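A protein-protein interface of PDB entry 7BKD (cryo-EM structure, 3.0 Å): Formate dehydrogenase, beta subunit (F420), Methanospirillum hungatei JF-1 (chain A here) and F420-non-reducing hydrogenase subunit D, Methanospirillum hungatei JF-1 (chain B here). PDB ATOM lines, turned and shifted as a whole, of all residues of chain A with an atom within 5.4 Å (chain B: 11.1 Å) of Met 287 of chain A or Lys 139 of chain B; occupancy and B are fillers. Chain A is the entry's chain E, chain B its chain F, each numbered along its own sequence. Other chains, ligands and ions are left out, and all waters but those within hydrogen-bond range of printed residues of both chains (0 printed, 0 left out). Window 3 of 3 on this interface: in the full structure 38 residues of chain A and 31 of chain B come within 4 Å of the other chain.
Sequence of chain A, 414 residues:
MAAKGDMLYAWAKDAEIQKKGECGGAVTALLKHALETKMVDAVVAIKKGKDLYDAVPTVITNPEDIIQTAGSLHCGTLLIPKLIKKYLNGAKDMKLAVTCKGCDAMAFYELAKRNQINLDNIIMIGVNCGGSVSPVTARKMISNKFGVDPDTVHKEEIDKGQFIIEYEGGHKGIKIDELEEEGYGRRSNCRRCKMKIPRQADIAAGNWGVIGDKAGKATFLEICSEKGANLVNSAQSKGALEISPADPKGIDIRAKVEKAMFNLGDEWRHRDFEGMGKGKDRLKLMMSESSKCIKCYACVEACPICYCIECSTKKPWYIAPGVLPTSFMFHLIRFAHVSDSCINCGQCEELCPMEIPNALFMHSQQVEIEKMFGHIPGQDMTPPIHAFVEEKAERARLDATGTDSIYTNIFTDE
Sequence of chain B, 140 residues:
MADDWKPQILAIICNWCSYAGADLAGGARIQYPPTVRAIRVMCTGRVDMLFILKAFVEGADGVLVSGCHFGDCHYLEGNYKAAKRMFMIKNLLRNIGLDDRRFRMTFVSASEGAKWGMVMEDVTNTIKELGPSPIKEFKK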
ATOM      1  N   ARG A 282      -3.960   7.230  10.584  1.00  0.00           N
ATOM      2  CA  ARG A 282      -4.315   5.819  10.500  1.00  0.00           C
ATOM      3  C   ARG A 282      -5.819   5.621  10.618  1.00  0.00           C
ATOM      4  O   ARG A 282      -6.402   4.791   9.910  1.00  0.00           O
ATOM      5  CB  ARG A 282      -3.592   5.025  11.581  1.00  0.00           C
ATOM      6  CG  ARG A 282      -3.737   3.533  11.423  1.00  0.00           C
ATOM      7  CD  ARG A 282      -3.184   2.804  12.617  1.00  0.00           C
ATOM      8  NE  ARG A 282      -1.808   2.372  12.413  1.00  0.00           N
ATOM      9  CZ  ARG A 282      -1.299   1.256  12.917  1.00  0.00           C
ATOM     10  NH1 ARG A 282      -2.057   0.456  13.650  1.00  0.00           N
ATOM     11  NH2 ARG A 282      -0.035   0.937  12.687  1.00  0.00           N
ATOM     12  N   LEU A 283      -6.464   6.364  11.519  1.00  0.00           N
ATOM     13  CA  LEU A 283      -7.914   6.286  11.638  1.00  0.00           C
ATOM     14  C   LEU A 283      -8.591   6.731  10.355  1.00  0.00           C
ATOM     15  O   LEU A 283      -9.554   6.104   9.901  1.00  0.00           O
ATOM     16  CB  LEU A 283      -8.392   7.142  12.809  1.00  0.00           C
ATOM     17  CG  LEU A 283      -9.888   7.100  13.120  1.00  0.00           C
ATOM     18  CD1 LEU A 283     -10.262   5.825  13.851  1.00  0.00           C
ATOM     19  CD2 LEU A 283     -10.300   8.318  13.909  1.00  0.00           C
ATOM     20  N   LYS A 284      -8.104   7.818   9.758  1.00  0.00           N
ATOM     21  CA  LYS A 284      -8.680   8.288   8.506  1.00  0.00           C
ATOM     22  C   LYS A 284      -8.515   7.247   7.409  1.00  0.00           C
ATOM     23  O   LYS A 284      -9.450   6.990   6.643  1.00  0.00           O
ATOM     24  CB  LYS A 284      -8.032   9.611   8.104  1.00  0.00           C
ATOM     25  CG  LYS A 284      -8.596  10.224   6.844  1.00  0.00           C
ATOM     26  CD  LYS A 284      -7.978  11.582   6.579  1.00  0.00           C
ATOM     27  CE  LYS A 284      -8.429  12.139   5.241  1.00  0.00           C
ATOM     28  NZ  LYS A 284      -9.888  12.435   5.235  1.00  0.00           N
ATOM     29  N   LEU A 285      -7.338   6.625   7.333  1.00  0.00           N
ATOM     30  CA  LEU A 285      -7.109   5.571   6.354  1.00  0.00           C
ATOM     31  C   LEU A 285      -8.080   4.417   6.541  1.00  0.00           C
ATOM     32  O   LEU A 285      -8.719   3.972   5.582  1.00  0.00           O
ATOM     33  CB  LEU A 285      -5.673   5.063   6.449  1.00  0.00           C
ATOM     34  CG  LEU A 285      -5.362   3.892   5.518  1.00  0.00           C
ATOM     35  CD1 LEU A 285      -5.477   4.304   4.062  1.00  0.00           C
ATOM     36  CD2 LEU A 285      -3.994   3.314   5.814  1.00  0.00           C
ATOM     37  N   MET A 286      -8.197   3.906   7.768  1.00  0.00           N
ATOM     38  CA  MET A 286      -9.068   2.755   7.986  1.00  0.00           C
ATOM     39  C   MET A 286     -10.525   3.088   7.707  1.00  0.00           C
ATOM     40  O   MET A 286     -11.240   2.280   7.108  1.00  0.00           O
ATOM     41  CB  MET A 286      -8.911   2.194   9.398  1.00  0.00           C
ATOM     42  CG  MET A 286      -7.569   1.556   9.669  1.00  0.00           C
ATOM     43  SD  MET A 286      -7.442   0.913  11.342  1.00  0.00           S
ATOM     44  CE  MET A 286      -5.751   0.334  11.345  1.00  0.00           C
ATOM     45  N   MET A 287     -10.993   4.258   8.133  1.00  0.00           N
ATOM     46  CA  MET A 287     -12.396   4.578   7.896  1.00  0.00           C
ATOM     47  C   MET A 287     -12.674   4.805   6.416  1.00  0.00           C
ATOM     48  O   MET A 287     -13.703   4.349   5.901  1.00  0.00           O
ATOM     49  CB  MET A 287     -12.817   5.784   8.730  1.00  0.00           C
ATOM     50  CG  MET A 287     -12.817   5.506  10.223  1.00  0.00           C
ATOM     51  SD  MET A 287     -13.257   6.935  11.213  1.00  0.00           S
ATOM     52  CE  MET A 287     -14.995   7.064  10.818  1.00  0.00           C
ATOM     53  N   SER A 288     -11.765   5.478   5.707  1.00  0.00           N
ATOM     54  CA  SER A 288     -11.951   5.664   4.273  1.00  0.00           C
ATOM     55  C   SER A 288     -11.942   4.333   3.538  1.00  0.00           C
ATOM     56  O   SER A 288     -12.738   4.120   2.618  1.00  0.00           O
ATOM     57  CB  SER A 288     -10.870   6.589   3.719  1.00  0.00           C
ATOM     58  OG  SER A 288     -11.206   7.948   3.929  1.00  0.00           O
ATOM     59  N   GLU A 289     -11.043   3.426   3.922  1.00  0.00           N
ATOM     60  CA  GLU A 289     -11.009   2.111   3.294  1.00  0.00           C
ATOM     61  C   GLU A 289     -12.290   1.339   3.567  1.00  0.00           C
ATOM     62  O   GLU A 289     -12.911   0.805   2.645  1.00  0.00           O
ATOM     63  CB  GLU A 289      -9.799   1.324   3.788  1.00  0.00           C
ATOM     64  CG  GLU A 289      -8.543   1.570   2.991  1.00  0.00           C
ATOM     65  CD  GLU A 289      -8.802   1.574   1.504  1.00  0.00           C
ATOM     66  OE1 GLU A 289      -9.198   0.518   0.970  1.00  0.00           O
ATOM     67  OE2 GLU A 289      -8.610   2.631   0.868  1.00  0.00           O
ATOM     68  N   SER A 290     -12.711   1.283   4.826  1.00  0.00           N
ATOM     69  CA  SER A 290     -13.872   0.488   5.191  1.00  0.00           C
ATOM     70  C   SER A 290     -15.183   1.102   4.732  1.00  0.00           C
ATOM     71  O   SER A 290     -16.206   0.415   4.768  1.00  0.00           O
ATOM     72  CB  SER A 290     -13.895   0.281   6.703  1.00  0.00           C
ATOM     73  OG  SER A 290     -12.705  -0.347   7.141  1.00  0.00           O
ATOM     74  N   SER A 291     -15.190   2.366   4.311  1.00  0.00           N
ATOM     75  CA  SER A 291     -16.421   2.939   3.786  1.00  0.00           C
ATOM     76  C   SER A 291     -16.858   2.286   2.483  1.00  0.00           C
ATOM     77  O   SER A 291     -18.017   2.438   2.089  1.00  0.00           O
ATOM     78  CB  SER A 291     -16.260   4.442   3.575  1.00  0.00           C
ATOM     79  OG  SER A 291     -15.359   4.711   2.519  1.00  0.00           O
ATOM     80  N   PHE A 328     -18.601   2.408  10.544  1.00  0.00           N
ATOM     81  CA  PHE A 328     -17.314   1.832  10.902  1.00  0.00           C
ATOM     82  C   PHE A 328     -17.459   0.678  11.880  1.00  0.00           C
ATOM     83  O   PHE A 328     -16.500  -0.068  12.085  1.00  0.00           O
ATOM     84  CB  PHE A 328     -16.421   2.930  11.480  1.00  0.00           C
ATOM     85  CG  PHE A 328     -15.004   2.510  11.718  1.00  0.00           C
ATOM     86  CD1 PHE A 328     -14.337   2.910  12.859  1.00  0.00           C
ATOM     87  CD2 PHE A 328     -14.334   1.728  10.803  1.00  0.00           C
ATOM     88  CE1 PHE A 328     -13.035   2.530  13.085  1.00  0.00           C
ATOM     89  CE2 PHE A 328     -13.031   1.345  11.026  1.00  0.00           C
ATOM     90  CZ  PHE A 328     -12.382   1.748  12.167  1.00  0.00           C
ATOM     91  N   LEU B  53     -17.340  -0.058  21.746  1.00  0.00           N
ATOM     92  CA  LEU B  53     -17.082   0.323  20.363  1.00  0.00           C
ATOM     93  C   LEU B  53     -18.275   1.041  19.747  1.00  0.00           C
ATOM     94  O   LEU B  53     -18.103   1.998  18.988  1.00  0.00           O
ATOM     95  CB  LEU B  53     -16.701  -0.910  19.552  1.00  0.00           C
ATOM     96  CG  LEU B  53     -15.394  -1.538  20.031  1.00  0.00           C
ATOM     97  CD1 LEU B  53     -15.193  -2.900  19.416  1.00  0.00           C
ATOM     98  CD2 LEU B  53     -14.235  -0.626  19.705  1.00  0.00           C
ATOM     99  N   PHE B  56     -18.225   4.562  21.020  1.00  0.00           N
ATOM    100  CA  PHE B  56     -17.217   5.385  20.358  1.00  0.00           C
ATOM    101  C   PHE B  56     -17.615   5.725  18.929  1.00  0.00           C
ATOM    102  O   PHE B  56     -17.344   6.830  18.450  1.00  0.00           O
ATOM    103  CB  PHE B  56     -15.865   4.683  20.392  1.00  0.00           C
ATOM    104  CG  PHE B  56     -15.073   4.988  21.618  1.00  0.00           C
ATOM    105  CD1 PHE B  56     -14.714   6.288  21.916  1.00  0.00           C
ATOM    106  CD2 PHE B  56     -14.715   3.984  22.492  1.00  0.00           C
ATOM    107  CE1 PHE B  56     -13.997   6.576  23.045  1.00  0.00           C
ATOM    108  CE2 PHE B  56     -14.001   4.267  23.626  1.00  0.00           C
ATOM    109  CZ  PHE B  56     -13.638   5.564  23.903  1.00  0.00           C
ATOM    110  N   VAL B  57     -18.250   4.786  18.229  1.00  0.00           N
ATOM    111  CA  VAL B  57     -18.692   5.043  16.863  1.00  0.00           C
ATOM    112  C   VAL B  57     -19.824   6.061  16.842  1.00  0.00           C
ATOM    113  O   VAL B  57     -19.846   6.965  15.999  1.00  0.00           O
ATOM    114  CB  VAL B  57     -19.104   3.725  16.184  1.00  0.00           C
ATOM    115  CG1 VAL B  57     -19.949   4.001  14.961  1.00  0.00           C
ATOM    116  CG2 VAL B  57     -17.880   2.937  15.799  1.00  0.00           C
ATOM    117  N   GLU B  58     -20.778   5.937  17.767  1.00  0.00           N
ATOM    118  CA  GLU B  58     -21.955   6.798  17.750  1.00  0.00           C
ATOM    119  C   GLU B  58     -21.629   8.250  18.073  1.00  0.00           C
ATOM    120  O   GLU B  58     -22.468   9.124  17.832  1.00  0.00           O
ATOM    121  CB  GLU B  58     -23.002   6.271  18.728  1.00  0.00           C
ATOM    122  CG  GLU B  58     -23.748   5.042  18.243  1.00  0.00           C
ATOM    123  CD  GLU B  58     -24.712   5.346  17.115  1.00  0.00           C
ATOM    124  OE1 GLU B  58     -25.892   5.637  17.403  1.00  0.00           O
ATOM    125  OE2 GLU B  58     -24.293   5.286  15.940  1.00  0.00           O
ATOM    126  N   GLY B  59     -20.447   8.530  18.610  1.00  0.00           N
ATOM    127  CA  GLY B  59     -20.045   9.902  18.833  1.00  0.00           C
ATOM    128  C   GLY B  59     -19.594  10.214  20.243  1.00  0.00           C
ATOM    129  O   GLY B  59     -19.560  11.381  20.638  1.00  0.00           O
ATOM    130  N   LEU B  92      -7.030  -1.926  21.014  1.00  0.00           N
ATOM    131  CA  LEU B  92      -7.755  -1.700  19.772  1.00  0.00           C
ATOM    132  C   LEU B  92      -7.853  -0.214  19.454  1.00  0.00           C
ATOM    133  O   LEU B  92      -7.620   0.198  18.313  1.00  0.00           O
ATOM    134  CB  LEU B  92      -9.139  -2.341  19.865  1.00  0.00           C
ATOM    135  CG  LEU B  92     -10.034  -2.433  18.630  1.00  0.00           C
ATOM    136  CD1 LEU B  92     -10.955  -3.615  18.791  1.00  0.00           C
ATOM    137  CD2 LEU B  92     -10.843  -1.171  18.411  1.00  0.00           C
ATOM    138  N   LEU B  93      -8.183   0.609  20.451  1.00  0.00           N
ATOM    139  CA  LEU B  93      -8.259   2.048  20.211  1.00  0.00           C
ATOM    140  C   LEU B  93      -6.908   2.658  19.874  1.00  0.00           C
ATOM    141  O   LEU B  93      -6.848   3.611  19.092  1.00  0.00           O
ATOM    142  CB  LEU B  93      -8.900   2.787  21.385  1.00  0.00           C
ATOM    143  CG  LEU B  93     -10.419   2.773  21.538  1.00  0.00           C
ATOM    144  CD1 LEU B  93     -11.006   1.462  21.957  1.00  0.00           C
ATOM    145  CD2 LEU B  93     -10.773   3.853  22.539  1.00  0.00           C
ATOM    146  N   ASN B  95      -4.507   0.992  18.196  1.00  0.00           N
ATOM    147  CA  ASN B  95      -4.083   0.491  16.896  1.00  0.00           C
ATOM    148  C   ASN B  95      -4.991   0.938  15.763  1.00  0.00           C
ATOM    149  O   ASN B  95      -4.605   0.808  14.600  1.00  0.00           O
ATOM    150  CB  ASN B  95      -4.005  -1.029  16.927  1.00  0.00           C
ATOM    151  CG  ASN B  95      -2.844  -1.524  17.741  1.00  0.00           C
ATOM    152  OD1 ASN B  95      -1.743  -0.990  17.655  1.00  0.00           O
ATOM    153  ND2 ASN B  95      -3.082  -2.544  18.549  1.00  0.00           N
ATOM    154  N   ILE B  96      -6.189   1.449  16.062  1.00  0.00           N
ATOM    155  CA  ILE B  96      -7.024   2.017  15.010  1.00  0.00           C
ATOM    156  C   ILE B  96      -6.813   3.512  14.848  1.00  0.00           C
ATOM    157  O   ILE B  96      -7.514   4.140  14.045  1.00  0.00           O
ATOM    158  CB  ILE B  96      -8.524   1.753  15.243  1.00  0.00           C
ATOM    159  CG1 ILE B  96      -9.007   2.469  16.502  1.00  0.00           C
ATOM    160  CG2 ILE B  96      -8.800   0.266  15.313  1.00  0.00           C
ATOM    161  CD1 ILE B  96     -10.500   2.636  16.567  1.00  0.00           C
ATOM    162  N   GLY B  97      -5.873   4.103  15.578  1.00  0.00           N
ATOM    163  CA  GLY B  97      -5.582   5.513  15.462  1.00  0.00           C
ATOM    164  C   GLY B  97      -6.314   6.407  16.438  1.00  0.00           C
ATOM    165  O   GLY B  97      -6.041   7.612  16.468  1.00  0.00           O
ATOM    166  N   LEU B  98      -7.233   5.866  17.227  1.00  0.00           N
ATOM    167  CA  LEU B  98      -7.892   6.662  18.247  1.00  0.00           C
ATOM    168  C   LEU B  98      -6.954   6.864  19.433  1.00  0.00           C
ATOM    169  O   LEU B  98      -5.964   6.150  19.602  1.00  0.00           O
ATOM    170  CB  LEU B  98      -9.183   5.985  18.696  1.00  0.00           C
ATOM    171  CG  LEU B  98     -10.289   6.880  19.246  1.00  0.00           C
ATOM    172  CD1 LEU B  98     -10.773   7.821  18.168  1.00  0.00           C
ATOM    173  CD2 LEU B  98     -11.434   6.037  19.757  1.00  0.00           C
ATOM    174  N   ASP B  99      -7.264   7.861  20.255  1.00  0.00           N
ATOM    175  CA  ASP B  99      -6.467   8.121  21.447  1.00  0.00           C
ATOM    176  C   ASP B  99      -6.938   7.184  22.550  1.00  0.00           C
ATOM    177  O   ASP B  99      -8.060   7.313  23.044  1.00  0.00           O
ATOM    178  CB  ASP B  99      -6.587   9.580  21.871  1.00  0.00           C
ATOM    179  CG  ASP B  99      -5.524   9.984  22.873  1.00  0.00           C
ATOM    180  OD1 ASP B  99      -4.356  10.158  22.468  1.00  0.00           O
ATOM    181  OD2 ASP B  99      -5.850  10.125  24.067  1.00  0.00           O
ATOM    182  N   SER B 133     -14.018  13.857  19.517  1.00  0.00           N
ATOM    183  CA  SER B 133     -13.558  12.635  18.877  1.00  0.00           C
ATOM    184  C   SER B 133     -13.276  12.884  17.399  1.00  0.00           C
ATOM    185  O   SER B 133     -14.061  13.557  16.721  1.00  0.00           O
ATOM    186  CB  SER B 133     -14.596  11.524  19.016  1.00  0.00           C
ATOM    187  OG  SER B 133     -14.646  11.033  20.339  1.00  0.00           O
ATOM    188  N   PRO B 134     -12.170  12.364  16.871  1.00  0.00           N
ATOM    189  CA  PRO B 134     -11.933  12.478  15.426  1.00  0.00           C
ATOM    190  C   PRO B 134     -12.967  11.748  14.598  1.00  0.00           C
ATOM    191  O   PRO B 134     -13.213  12.134  13.449  1.00  0.00           O
ATOM    192  CB  PRO B 134     -10.539  11.864  15.256  1.00  0.00           C
ATOM    193  CG  PRO B 134     -10.400  10.938  16.407  1.00  0.00           C
ATOM    194  CD  PRO B 134     -11.136  11.563  17.544  1.00  0.00           C
ATOM    195  N   ILE B 135     -13.583  10.703  15.155  1.00  0.00           N
ATOM    196  CA  ILE B 135     -14.512   9.873  14.398  1.00  0.00           C
ATOM    197  C   ILE B 135     -15.724  10.672  13.946  1.00  0.00           C
ATOM    198  O   ILE B 135     -16.339  10.355  12.922  1.00  0.00           O
ATOM    199  CB  ILE B 135     -14.913   8.647  15.241  1.00  0.00           C
ATOM    200  CG1 ILE B 135     -13.676   7.834  15.600  1.00  0.00           C
ATOM    201  CG2 ILE B 135     -15.893   7.770  14.496  1.00  0.00           C
ATOM    202  CD1 ILE B 135     -13.963   6.634  16.460  1.00  0.00           C
ATOM    203  N   LYS B 136     -16.091  11.719  14.685  1.00  0.00           N
ATOM    204  CA  LYS B 136     -17.237  12.528  14.283  1.00  0.00           C
ATOM    205  C   LYS B 136     -16.965  13.275  12.982  1.00  0.00           C
ATOM    206  O   LYS B 136     -17.858  13.402  12.137  1.00  0.00           O
ATOM    207  CB  LYS B 136     -17.606  13.506  15.395  1.00  0.00           C
ATOM    208  CG  LYS B 136     -18.759  13.040  16.258  1.00  0.00           C
ATOM    209  CD  LYS B 136     -18.894  13.895  17.503  1.00  0.00           C
ATOM    210  CE  LYS B 136     -18.028  13.369  18.630  1.00  0.00           C
ATOM    211  NZ  LYS B 136     -18.423  13.950  19.935  1.00  0.00           N
ATOM    212  N   GLU B 137     -15.745  13.786  12.808  1.00  0.00           N
ATOM    213  CA  GLU B 137     -15.411  14.511  11.585  1.00  0.00           C
ATOM    214  C   GLU B 137     -15.412  13.585  10.376  1.00  0.00           C
ATOM    215  O   GLU B 137     -16.040  13.882   9.353  1.00  0.00           O
ATOM    216  CB  GLU B 137     -14.054  15.196  11.736  1.00  0.00           C
ATOM    217  CG  GLU B 137     -13.615  15.973  10.507  1.00  0.00           C
ATOM    218  CD  GLU B 137     -12.365  16.795  10.754  1.00  0.00           C
ATOM    219  OE1 GLU B 137     -11.837  16.753  11.885  1.00  0.00           O
ATOM    220  OE2 GLU B 137     -11.912  17.487   9.817  1.00  0.00           O
ATOM    221  N   PHE B 138     -14.713  12.458  10.473  1.00  0.00           N
ATOM    222  CA  PHE B 138     -14.730  11.476   9.400  1.00  0.00           C
ATOM    223  C   PHE B 138     -16.116  10.857   9.291  1.00  0.00           C
ATOM    224  O   PHE B 138     -16.759  10.562  10.300  1.00  0.00           O
ATOM    225  CB  PHE B 138     -13.680  10.397   9.651  1.00  0.00           C
ATOM    226  CG  PHE B 138     -12.319  10.944   9.957  1.00  0.00           C
ATOM    227  CD1 PHE B 138     -11.823  12.030   9.261  1.00  0.00           C
ATOM    228  CD2 PHE B 138     -11.538  10.375  10.943  1.00  0.00           C
ATOM    229  CE1 PHE B 138     -10.573  12.538   9.543  1.00  0.00           C
ATOM    230  CE2 PHE B 138     -10.288  10.879  11.230  1.00  0.00           C
ATOM    231  CZ  PHE B 138      -9.805  11.962  10.529  1.00  0.00           C
ATOM    232  N   LYS B 139     -16.578  10.669   8.060  1.00  0.00           N
ATOM    233  CA  LYS B 139     -17.945  10.216   7.841  1.00  0.00           C
ATOM    234  C   LYS B 139     -18.189   8.884   8.535  1.00  0.00           C
ATOM    235  O   LYS B 139     -17.616   7.858   8.158  1.00  0.00           O
ATOM    236  CB  LYS B 139     -18.226  10.107   6.344  1.00  0.00           C
ATOM    237  CG  LYS B 139     -18.130  11.435   5.602  1.00  0.00           C
ATOM    238  CD  LYS B 139     -19.306  12.348   5.934  1.00  0.00           C
ATOM    239  CE  LYS B 139     -18.891  13.486   6.857  1.00  0.00           C
ATOM    240  NZ  LYS B 139     -20.016  14.419   7.133  1.00  0.00           N
ATOM    241  N   LYS B 140     -19.038   8.911   9.556  1.00  0.00           N
ATOM    242  CA  LYS B 140     -19.347   7.727  10.348  1.00  0.00           C
ATOM    243  C   LYS B 140     -20.712   7.157   9.975  1.00  0.00           C
ATOM    244  O   LYS B 140     -21.611   7.891   9.566  1.00  0.00           O
ATOM    245  CB  LYS B 140     -19.306   8.062  11.840  1.00  0.00           C
ATOM    246  CG  LYS B 140     -20.342   9.090  12.269  1.00  0.00           C
ATOM    247  CD  LYS B 140     -20.244   9.402  13.751  1.00  0.00           C
ATOM    248  CE  LYS B 140     -21.271  10.448  14.156  1.00  0.00           C
ATOM    249  NZ  LYS B 140     -21.191  10.785  15.604  1.00  0.00           N
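The guanidinium group of Arg 282 of chain A lies within hydrogen-bond range of the backbone carbonyl oxygen of Asn 95 of chain B (2.7 Å).
Of the 20 printed residues of chain B, 6 touch a printed residue of chain A. Hydrophobic or aromatic side chains of chain B that line the printed part of chain A: Pro 134, Ile 135 and Phe 138. Hydrophobic or aromatic side chains of chain A that line the printed part of chain B: Leu 283, Met 286 and Met 287. Among the printed residues, 11 pairs touch across the chains. Among the printed residues, no Asp or Glu carboxylate lies within 4 Å of a Lys or Arg side-chain nitrogen of the other chain.
Ile 96 of chain B touches Leu 283 of chain A (O to CD1, 3.2 Å). Leu 283 of chain A touches Pro 134 of chain B. Leu 283 of chain A touches Ile 135 of chain B (CD2 to CG1, 3.8 Å). Leu 283 of chain A touches Phe 138 of chain B. Phe 138 of chain B touches Lys 284 of chain A (CZ to CB, 3.8 Å). Met 286 of chain A touches Asn 95 of chain B (CE to O, 3.5 Å). Met 286 of chain A touches Ile 96 of chain B. Met 287 of chain A touches Ile 135 of chain B. Met 287 of chain A touches Phe 138 of chain B (CE to CB, 3.8 Å). Met 287 of chain A touches Lys 139 of chain B.
Printed residues of chain B within 4 Å of Arg 282 of chain A: Asn 95. Of the printed residues of chain B, Leu 283 of chain A touches Ile 96, Pro 134, Ile 135 and Phe 138. Of the printed residues of chain B, Lys 284 of chain A touches Phe 138. Met 287 of chain A touches three residues of chain B. Ser 291 of chain A touches none of the printed residues of chain B. Phe 328 of chain A touches none of the printed residues of chain B. Phe 56 of chain B touches none of the printed residues of chain A. Of the printed residues of chain A, Ile 96 of chain B touches Leu 283 (3.2 Å) and Met 286 (3.9 Å). Of the printed residues of chain A, Pro 134 of chain B touches Leu 283. Lys 139 of chain B touches one residue of chain A. The nearest residue of chain B that does not touch Met 287 of chain A is Lys 140 of chain B (4.4 Å). The nearest printed residue of chain A that does not touch Lys 139 of chain B is Ser 291 of chain A (5.9 Å). The nearest printed residue of chain B that does not touch Lys 284 of chain A is Ile 96 of chain B (5.7 Å).
The side-chain hydroxyl of Ser 288 of chain A sits close to the backbone carbonyl oxygen of Lys 284 of chain A (3.4 Å). OG of Ser 290 of chain A is in hydrogen-bond range of O of Met 286 of chain A, at 3.0 Å.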
